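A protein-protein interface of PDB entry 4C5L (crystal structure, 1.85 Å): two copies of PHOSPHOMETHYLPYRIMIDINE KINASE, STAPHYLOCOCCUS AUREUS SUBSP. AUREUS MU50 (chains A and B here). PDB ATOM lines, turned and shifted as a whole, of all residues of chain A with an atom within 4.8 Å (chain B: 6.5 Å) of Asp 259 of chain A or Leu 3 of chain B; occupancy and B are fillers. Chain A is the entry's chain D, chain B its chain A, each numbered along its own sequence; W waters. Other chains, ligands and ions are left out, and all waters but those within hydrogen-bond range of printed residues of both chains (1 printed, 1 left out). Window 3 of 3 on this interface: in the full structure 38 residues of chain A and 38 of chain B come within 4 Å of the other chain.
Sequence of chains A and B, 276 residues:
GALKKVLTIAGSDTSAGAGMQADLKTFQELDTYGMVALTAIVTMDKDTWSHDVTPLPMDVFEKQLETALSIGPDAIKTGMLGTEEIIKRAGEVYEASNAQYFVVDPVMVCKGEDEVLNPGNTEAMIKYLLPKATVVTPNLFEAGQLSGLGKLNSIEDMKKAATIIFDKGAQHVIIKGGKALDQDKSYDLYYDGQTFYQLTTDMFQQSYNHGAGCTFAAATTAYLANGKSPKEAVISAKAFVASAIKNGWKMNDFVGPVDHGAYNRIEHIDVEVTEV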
ATOM      1  N   ALA A 244      16.049 -26.944 -10.945  1.00  0.00           N
ATOM      2  CA  ALA A 244      16.686 -26.981  -9.623  1.00  0.00           C
ATOM      3  C   ALA A 244      16.699 -28.391  -9.073  1.00  0.00           C
ATOM      4  O   ALA A 244      17.728 -28.840  -8.534  1.00  0.00           O
ATOM      5  CB  ALA A 244      16.001 -26.032  -8.674  1.00  0.00           C
ATOM      6  N   ASN A 247      19.125 -30.862 -10.934  1.00  0.00           N
ATOM      7  CA  ASN A 247      20.525 -30.611 -10.625  1.00  0.00           C
ATOM      8  C   ASN A 247      20.801 -30.427  -9.142  1.00  0.00           C
ATOM      9  O   ASN A 247      21.773 -29.780  -8.768  1.00  0.00           O
ATOM     10  CB  ASN A 247      20.998 -29.383 -11.401  1.00  0.00           C
ATOM     11  CG  ASN A 247      21.028 -29.616 -12.899  1.00  0.00           C
ATOM     12  OD1 ASN A 247      21.982 -30.151 -13.388  1.00  0.00           O
ATOM     13  ND2 ASN A 247      19.980 -29.214 -13.621  1.00  0.00           N
ATOM     14  N   GLY A 248      19.916 -30.959  -8.304  1.00  0.00           N
ATOM     15  CA  GLY A 248      20.101 -30.998  -6.849  1.00  0.00           C
ATOM     16  C   GLY A 248      21.299 -31.883  -6.561  1.00  0.00           C
ATOM     17  O   GLY A 248      21.745 -32.593  -7.455  1.00  0.00           O
ATOM     18  N   TRP A 249      21.831 -31.824  -5.340  1.00  0.00           N
ATOM     19  CA  TRP A 249      23.061 -32.547  -4.987  1.00  0.00           C
ATOM     20  C   TRP A 249      22.982 -33.190  -3.585  1.00  0.00           C
ATOM     21  O   TRP A 249      22.231 -32.739  -2.730  1.00  0.00           O
ATOM     22  CB  TRP A 249      24.300 -31.613  -5.090  1.00  0.00           C
ATOM     23  CG  TRP A 249      24.206 -30.343  -4.273  1.00  0.00           C
ATOM     24  CD1 TRP A 249      23.612 -29.145  -4.656  1.00  0.00           C
ATOM     25  CD2 TRP A 249      24.712 -30.121  -2.948  1.00  0.00           C
ATOM     26  NE1 TRP A 249      23.734 -28.227  -3.647  1.00  0.00           N
ATOM     27  CE2 TRP A 249      24.377 -28.804  -2.586  1.00  0.00           C
ATOM     28  CE3 TRP A 249      25.381 -30.920  -2.015  1.00  0.00           C
ATOM     29  CZ2 TRP A 249      24.707 -28.282  -1.361  1.00  0.00           C
ATOM     30  CZ3 TRP A 249      25.702 -30.388  -0.806  1.00  0.00           C
ATOM     31  CH2 TRP A 249      25.399 -29.087  -0.497  1.00  0.00           C
ATOM     32  N   PRO A 257      19.778 -30.677  -1.288  1.00  0.00           N
ATOM     33  CA  PRO A 257      18.962 -29.559  -1.734  1.00  0.00           C
ATOM     34  C   PRO A 257      18.848 -29.448  -3.242  1.00  0.00           C
ATOM     35  O   PRO A 257      19.657 -29.960  -3.971  1.00  0.00           O
ATOM     36  CB  PRO A 257      19.714 -28.362  -1.218  1.00  0.00           C
ATOM     37  CG  PRO A 257      21.150 -28.805  -1.336  1.00  0.00           C
ATOM     38  CD  PRO A 257      21.138 -30.249  -0.917  1.00  0.00           C
ATOM     39  N   VAL A 258      17.840 -28.730  -3.685  1.00  0.00           N
ATOM     40  CA  VAL A 258      17.761 -28.352  -5.067  1.00  0.00           C
ATOM     41  C   VAL A 258      18.885 -27.349  -5.349  1.00  0.00           C
ATOM     42  O   VAL A 258      19.425 -26.720  -4.419  1.00  0.00           O
ATOM     43  CB  VAL A 258      16.389 -27.748  -5.366  1.00  0.00           C
ATOM     44  CG1 VAL A 258      15.299 -28.763  -5.046  1.00  0.00           C
ATOM     45  CG2 VAL A 258      16.158 -26.476  -4.576  1.00  0.00           C
ATOM     46  N   ASP A 259      19.262 -27.222  -6.619  1.00  0.00           N
ATOM     47  CA  ASP A 259      20.188 -26.183  -7.048  1.00  0.00           C
ATOM     48  C   ASP A 259      19.401 -24.987  -7.583  1.00  0.00           C
ATOM     49  O   ASP A 259      19.055 -24.946  -8.773  1.00  0.00           O
ATOM     50  CB  ASP A 259      21.154 -26.695  -8.119  1.00  0.00           C
ATOM     51  CG  ASP A 259      22.176 -25.645  -8.558  1.00  0.00           C
ATOM     52  OD1 ASP A 259      22.049 -24.429  -8.213  1.00  0.00           O
ATOM     53  OD2 ASP A 259      23.096 -26.027  -9.318  1.00  0.00           O
ATOM     54  N   HIS A 260      19.201 -23.996  -6.721  1.00  0.00           N
ATOM     55  CA  HIS A 260      18.323 -22.852  -7.021  1.00  0.00           C
ATOM     56  C   HIS A 260      18.783 -22.092  -8.258  1.00  0.00           C
ATOM     57  O   HIS A 260      17.960 -21.437  -8.922  1.00  0.00           O
ATOM     58  CB  HIS A 260      18.228 -21.876  -5.828  1.00  0.00           C
ATOM     59  CG  HIS A 260      18.017 -22.566  -4.517  1.00  0.00           C
ATOM     60  ND1 HIS A 260      19.029 -23.251  -3.871  1.00  0.00           N
ATOM     61  CD2 HIS A 260      16.901 -22.744  -3.768  1.00  0.00           C
ATOM     62  CE1 HIS A 260      18.543 -23.806  -2.774  1.00  0.00           C
ATOM     63  NE2 HIS A 260      17.249 -23.538  -2.705  1.00  0.00           N
ATOM     64  N   GLY A 261      20.087 -22.136  -8.532  1.00  0.00           N
ATOM     65  CA  GLY A 261      20.627 -21.474  -9.732  1.00  0.00           C
ATOM     66  C   GLY A 261      20.608 -22.249 -11.058  1.00  0.00           C
ATOM     67  O   GLY A 261      21.070 -21.729 -12.078  1.00  0.00           O
ATOM     68  N   ALA A 262      20.056 -23.466 -11.062  1.00  0.00           N
ATOM     69  CA  ALA A 262      20.145 -24.354 -12.235  1.00  0.00           C
ATOM     70  C   ALA A 262      19.448 -23.856 -13.495  1.00  0.00           C
ATOM     71  O   ALA A 262      19.947 -24.053 -14.587  1.00  0.00           O
ATOM     72  CB  ALA A 262      19.647 -25.744 -11.899  1.00  0.00           C
ATOM     73  N   ARG A 265      21.769 -21.263 -14.910  1.00  0.00           N
ATOM     74  CA  ARG A 265      23.181 -21.612 -15.122  1.00  0.00           C
ATOM     75  C   ARG A 265      23.388 -22.948 -15.872  1.00  0.00           C
ATOM     76  O   ARG A 265      24.398 -23.113 -16.559  1.00  0.00           O
ATOM     77  CB  ARG A 265      23.930 -21.604 -13.785  1.00  0.00           C
ATOM     78  CG  ARG A 265      25.286 -22.282 -13.798  1.00  0.00           C
ATOM     79  CD  ARG A 265      26.037 -22.110 -12.497  1.00  0.00           C
ATOM     80  NE  ARG A 265      25.148 -21.938 -11.358  1.00  0.00           N
ATOM     81  CZ  ARG A 265      24.522 -22.911 -10.676  1.00  0.00           C
ATOM     82  NH1 ARG A 265      24.682 -24.188 -10.979  1.00  0.00           N
ATOM     83  NH2 ARG A 265      23.752 -22.580  -9.652  1.00  0.00           N
ATOM     84  N   ILE A 266      22.434 -23.875 -15.762  1.00  0.00           N
ATOM     85  CA  ILE A 266      22.580 -25.209 -16.323  1.00  0.00           C
ATOM     86  C   ILE A 266      21.612 -25.500 -17.489  1.00  0.00           C
ATOM     87  O   ILE A 266      22.067 -25.766 -18.610  1.00  0.00           O
ATOM     88  CB  ILE A 266      22.504 -26.284 -15.225  1.00  0.00           C
ATOM     89  CG1 ILE A 266      23.570 -25.985 -14.144  1.00  0.00           C
ATOM     90  CG2 ILE A 266      22.712 -27.679 -15.826  1.00  0.00           C
ATOM     91  CD1 ILE A 266      23.555 -26.870 -12.897  1.00  0.00           C
ATOM     92  N   GLY B   1      31.555 -29.505 -11.633  1.00  0.00           N
ATOM     93  CA  GLY B   1      31.746 -30.057 -10.248  1.00  0.00           C
ATOM     94  C   GLY B   1      30.773 -29.430  -9.274  1.00  0.00           C
ATOM     95  O   GLY B   1      30.090 -28.464  -9.600  1.00  0.00           O
ATOM     96  N   ALA B   2      30.730 -29.963  -8.056  1.00  0.00           N
ATOM     97  CA  ALA B   2      29.799 -29.530  -7.036  1.00  0.00           C
ATOM     98  C   ALA B   2      29.942 -28.038  -6.666  1.00  0.00           C
ATOM     99  O   ALA B   2      31.043 -27.478  -6.714  1.00  0.00           O
ATOM    100  CB  ALA B   2      29.974 -30.414  -5.794  1.00  0.00           C
ATOM    101  N   LEU B   3      28.824 -27.399  -6.349  1.00  0.00           N
ATOM    102  CA  LEU B   3      28.824 -26.035  -5.819  1.00  0.00           C
ATOM    103  C   LEU B   3      29.681 -25.979  -4.537  1.00  0.00           C
ATOM    104  O   LEU B   3      29.589 -26.860  -3.674  1.00  0.00           O
ATOM    105  CB  LEU B   3      27.401 -25.562  -5.494  1.00  0.00           C
ATOM    106  CG  LEU B   3      26.379 -25.261  -6.600  1.00  0.00           C
ATOM    107  CD1 LEU B   3      24.985 -25.067  -6.023  1.00  0.00           C
ATOM    108  CD2 LEU B   3      26.718 -24.056  -7.494  1.00  0.00           C
ATOM    109  N   LYS B   4      30.503 -24.940  -4.414  1.00  0.00           N
ATOM    110  CA  LYS B   4      31.293 -24.744  -3.201  1.00  0.00           C
ATOM    111  C   LYS B   4      30.379 -24.260  -2.117  1.00  0.00           C
ATOM    112  O   LYS B   4      29.462 -23.449  -2.364  1.00  0.00           O
ATOM    113  CB  LYS B   4      32.432 -23.743  -3.393  1.00  0.00           C
ATOM    114  CG  LYS B   4      33.411 -24.118  -4.466  1.00  0.00           C
ATOM    115  CD  LYS B   4      34.350 -25.207  -3.975  1.00  0.00           C
ATOM    116  CE  LYS B   4      35.352 -25.601  -5.034  1.00  0.00           C
ATOM    117  NZ  LYS B   4      36.200 -26.697  -4.499  1.00  0.00           N
ATOM    118  N   LYS B   5      30.609 -24.761  -0.914  1.00  0.00           N
ATOM    119  CA  LYS B   5      29.767 -24.411   0.212  1.00  0.00           C
ATOM    120  C   LYS B   5      30.367 -23.316   1.073  1.00  0.00           C
ATOM    121  O   LYS B   5      31.406 -23.480   1.648  1.00  0.00           O
ATOM    122  CB  LYS B   5      29.467 -25.619   1.055  1.00  0.00           C
ATOM    123  CG  LYS B   5      28.672 -26.706   0.323  1.00  0.00           C
ATOM    124  CD  LYS B   5      28.868 -28.059   1.014  1.00  0.00           C
ATOM    125  CE  LYS B   5      30.232 -28.621   0.667  1.00  0.00           C
ATOM    126  NZ  LYS B   5      30.684 -29.754   1.502  1.00  0.00           N
ATOM    127  N   GLN B  28      24.952 -16.305  -4.126  1.00  0.00           N
ATOM    128  CA  GLN B  28      24.144 -16.873  -5.182  1.00  0.00           C
ATOM    129  C   GLN B  28      24.583 -16.358  -6.568  1.00  0.00           C
ATOM    130  O   GLN B  28      24.715 -17.125  -7.518  1.00  0.00           O
ATOM    131  CB  GLN B  28      22.665 -16.521  -4.941  1.00  0.00           C
ATOM    132  CG  GLN B  28      21.724 -17.260  -5.844  1.00  0.00           C
ATOM    133  CD  GLN B  28      21.806 -18.760  -5.655  1.00  0.00           C
ATOM    134  OE1 GLN B  28      21.996 -19.251  -4.553  1.00  0.00           O
ATOM    135  NE2 GLN B  28      21.619 -19.494  -6.730  1.00  0.00           N
ATOM    136  N   ASP B  31      27.613 -18.212  -7.928  1.00  0.00           N
ATOM    137  CA  ASP B  31      27.468 -19.640  -8.200  1.00  0.00           C
ATOM    138  C   ASP B  31      28.084 -20.498  -7.120  1.00  0.00           C
ATOM    139  O   ASP B  31      28.875 -21.405  -7.396  1.00  0.00           O
ATOM    140  CB  ASP B  31      28.064 -19.984  -9.580  1.00  0.00           C
ATOM    141  CG  ASP B  31      27.530 -19.085 -10.672  1.00  0.00           C
ATOM    142  OD1 ASP B  31      26.301 -18.866 -10.718  1.00  0.00           O
ATOM    143  OD2 ASP B  31      28.323 -18.583 -11.495  1.00  0.00           O
ATOM    144  N   THR B  32      27.760 -20.174  -5.869  1.00  0.00           N
ATOM    145  CA  THR B  32      28.240 -20.959  -4.743  1.00  0.00           C
ATOM    146  C   THR B  32      27.018 -21.277  -3.904  1.00  0.00           C
ATOM    147  O   THR B  32      25.985 -20.642  -4.067  1.00  0.00           O
ATOM    148  CB  THR B  32      29.223 -20.161  -3.869  1.00  0.00           C
ATOM    149  OG1 THR B  32      28.549 -19.012  -3.334  1.00  0.00           O
ATOM    150  CG2 THR B  32      30.440 -19.718  -4.650  1.00  0.00           C
ATOM    151  N   TYR B  33      27.133 -22.259  -3.016  1.00  0.00           N
ATOM    152  CA  TYR B  33      26.011 -22.616  -2.141  1.00  0.00           C
ATOM    153  C   TYR B  33      26.118 -21.893  -0.799  1.00  0.00           C
ATOM    154  O   TYR B  33      26.927 -22.245   0.055  1.00  0.00           O
ATOM    155  CB  TYR B  33      25.964 -24.123  -1.921  1.00  0.00           C
ATOM    156  CG  TYR B  33      24.775 -24.571  -1.106  1.00  0.00           C
ATOM    157  CD1 TYR B  33      23.510 -24.755  -1.709  1.00  0.00           C
ATOM    158  CD2 TYR B  33      24.893 -24.790   0.264  1.00  0.00           C
ATOM    159  CE1 TYR B  33      22.422 -25.159  -0.972  1.00  0.00           C
ATOM    160  CE2 TYR B  33      23.794 -25.218   1.006  1.00  0.00           C
ATOM    161  CZ  TYR B  33      22.579 -25.387   0.383  1.00  0.00           C
ATOM    162  OH  TYR B  33      21.525 -25.826   1.113  1.00  0.00           O
ATOM    163  N   ASP B  74      33.276 -24.960   2.615  1.00  0.00           N
ATOM    164  CA  ASP B  74      34.573 -24.866   1.943  1.00  0.00           C
ATOM    165  C   ASP B  74      35.247 -23.524   2.306  1.00  0.00           C
ATOM    166  O   ASP B  74      36.466 -23.357   2.180  1.00  0.00           O
ATOM    167  CB  ASP B  74      34.377 -24.977   0.427  1.00  0.00           C
ATOM    168  CG  ASP B  74      33.792 -26.331   0.018  1.00  0.00           C
ATOM    169  OD1 ASP B  74      34.430 -27.347   0.358  1.00  0.00           O
ATOM    170  OD2 ASP B  74      32.699 -26.368  -0.596  1.00  0.00           O
ATOM    171  N   ASN B 226      35.949 -20.570  -5.018  1.00  0.00           N
ATOM    172  CA  ASN B 226      35.931 -21.015  -6.416  1.00  0.00           C
ATOM    173  C   ASN B 226      37.311 -21.040  -7.083  1.00  0.00           C
ATOM    174  O   ASN B 226      37.409 -21.316  -8.282  1.00  0.00           O
ATOM    175  CB  ASN B 226      34.944 -20.163  -7.226  1.00  0.00           C
ATOM    176  CG  ASN B 226      33.485 -20.481  -6.895  1.00  0.00           C
ATOM    177  OD1 ASN B 226      33.147 -21.617  -6.578  1.00  0.00           O
ATOM    178  ND2 ASN B 226      32.609 -19.504  -7.058  1.00  0.00           N
HETATM  179  O   HOH W   1      23.760 -19.806  -9.385  1.00  0.00           O
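Printed residues of chain B within 4 Å of Trp 249 of chain A: Lys 5 and Tyr 33.
Of chain B, only Leu 3 (3.7 Å) comes within 4 Å of Asp 259 of chain A.
Of the printed residues of chain B, Arg 265 of chain A touches Leu 3 and Asp 31.
Ile 266 of chain A touches none of the printed residues of chain B.
Leu 3 of chain B touches just these residues of chain A: Asp 259 and Arg 265.
Of the printed residues of chain A, Asp 31 of chain B touches Arg 265.
Of the printed residues of chain A, Tyr 33 of chain B touches Trp 249 (3.7 Å) and Pro 257 (3.9 Å).
The nearest residue of chain A that does not touch Leu 3 of chain B is Trp 249 of chain A (4.1 Å).
The nearest printed residue of chain B that does not touch Trp 249 of chain A is Leu 3 of chain B (4.1 Å).
Lys 5 of chain B touches Trp 249 of chain A (CD to CH2, 3.9 Å).
Tyr 33 of chain B touches Trp 249 of chain A (CG to CZ2, 3.7 Å).
Tyr 33 of chain B touches Pro 257 of chain A.
Asp 259 of chain A touches Leu 3 of chain B.
NE2 of Gln 28 of chain B touches N of Gly 261 of chain A (3.5 Å).
Leu 3 of chain B touches Arg 265 of chain A.
O of Lys 5 of chain B lies within hydrogen-bond range of N of Asp 74 of chain B (2.6 Å).
The backbone carbonyl oxygen of Lys 4 of chain B lies within hydrogen-bond range of the backbone NH of Tyr 33 of chain B (2.7 Å).
The backbone NH (N) of Gly 261 of chain A lies within hydrogen-bond range of the side-chain carboxylate (OD1) of Asp 259 of chain A (3.0 Å).
The side-chain carboxylate (OD1) of Asp 259 of chain A is in salt-bridge range of the guanidinium group (NH2) of Arg 265 of chain A, at 2.9 Å.
O of Ala 244 of chain A lies within hydrogen-bond range of N of Asp 259 of chain A.
The backbone NH (N) of Trp 249 of chain A is in hydrogen-bond range of the backbone carbonyl oxygen (O) of Pro 257 of chain A, 3.2 Å away.
Water W1 lies within hydrogen-bond range of the guanidinium group (NH2) of Arg 265 of chain A (2.8 Å), the side-chain carboxylate (OD1) of Asp 31 of chain B (3.0 Å) and the backbone carbonyl oxygen (O) of Gln 28 of chain B (3.4 Å).
Of the 12 printed residues of chain A, 5 touch a printed residue of chain B.
Hydrophobic or aromatic side chains of chain A that line the printed part of chain B: Trp 249 and Pro 257.
Of the 11 printed residues of chain B, 5 touch a printed residue of chain A.
Among the printed residues, 7 pairs touch across the chains.
The side-chain carboxylate of Asp 31 of chain B lies within salt-bridge range of the guanidinium group of Arg 265 of chain A, at 3.3 Å.
No position is printed for both chains.
Of the 7 pairs that touch across the chains among the printed residues, none has its exchanged pair printed and touching as well.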
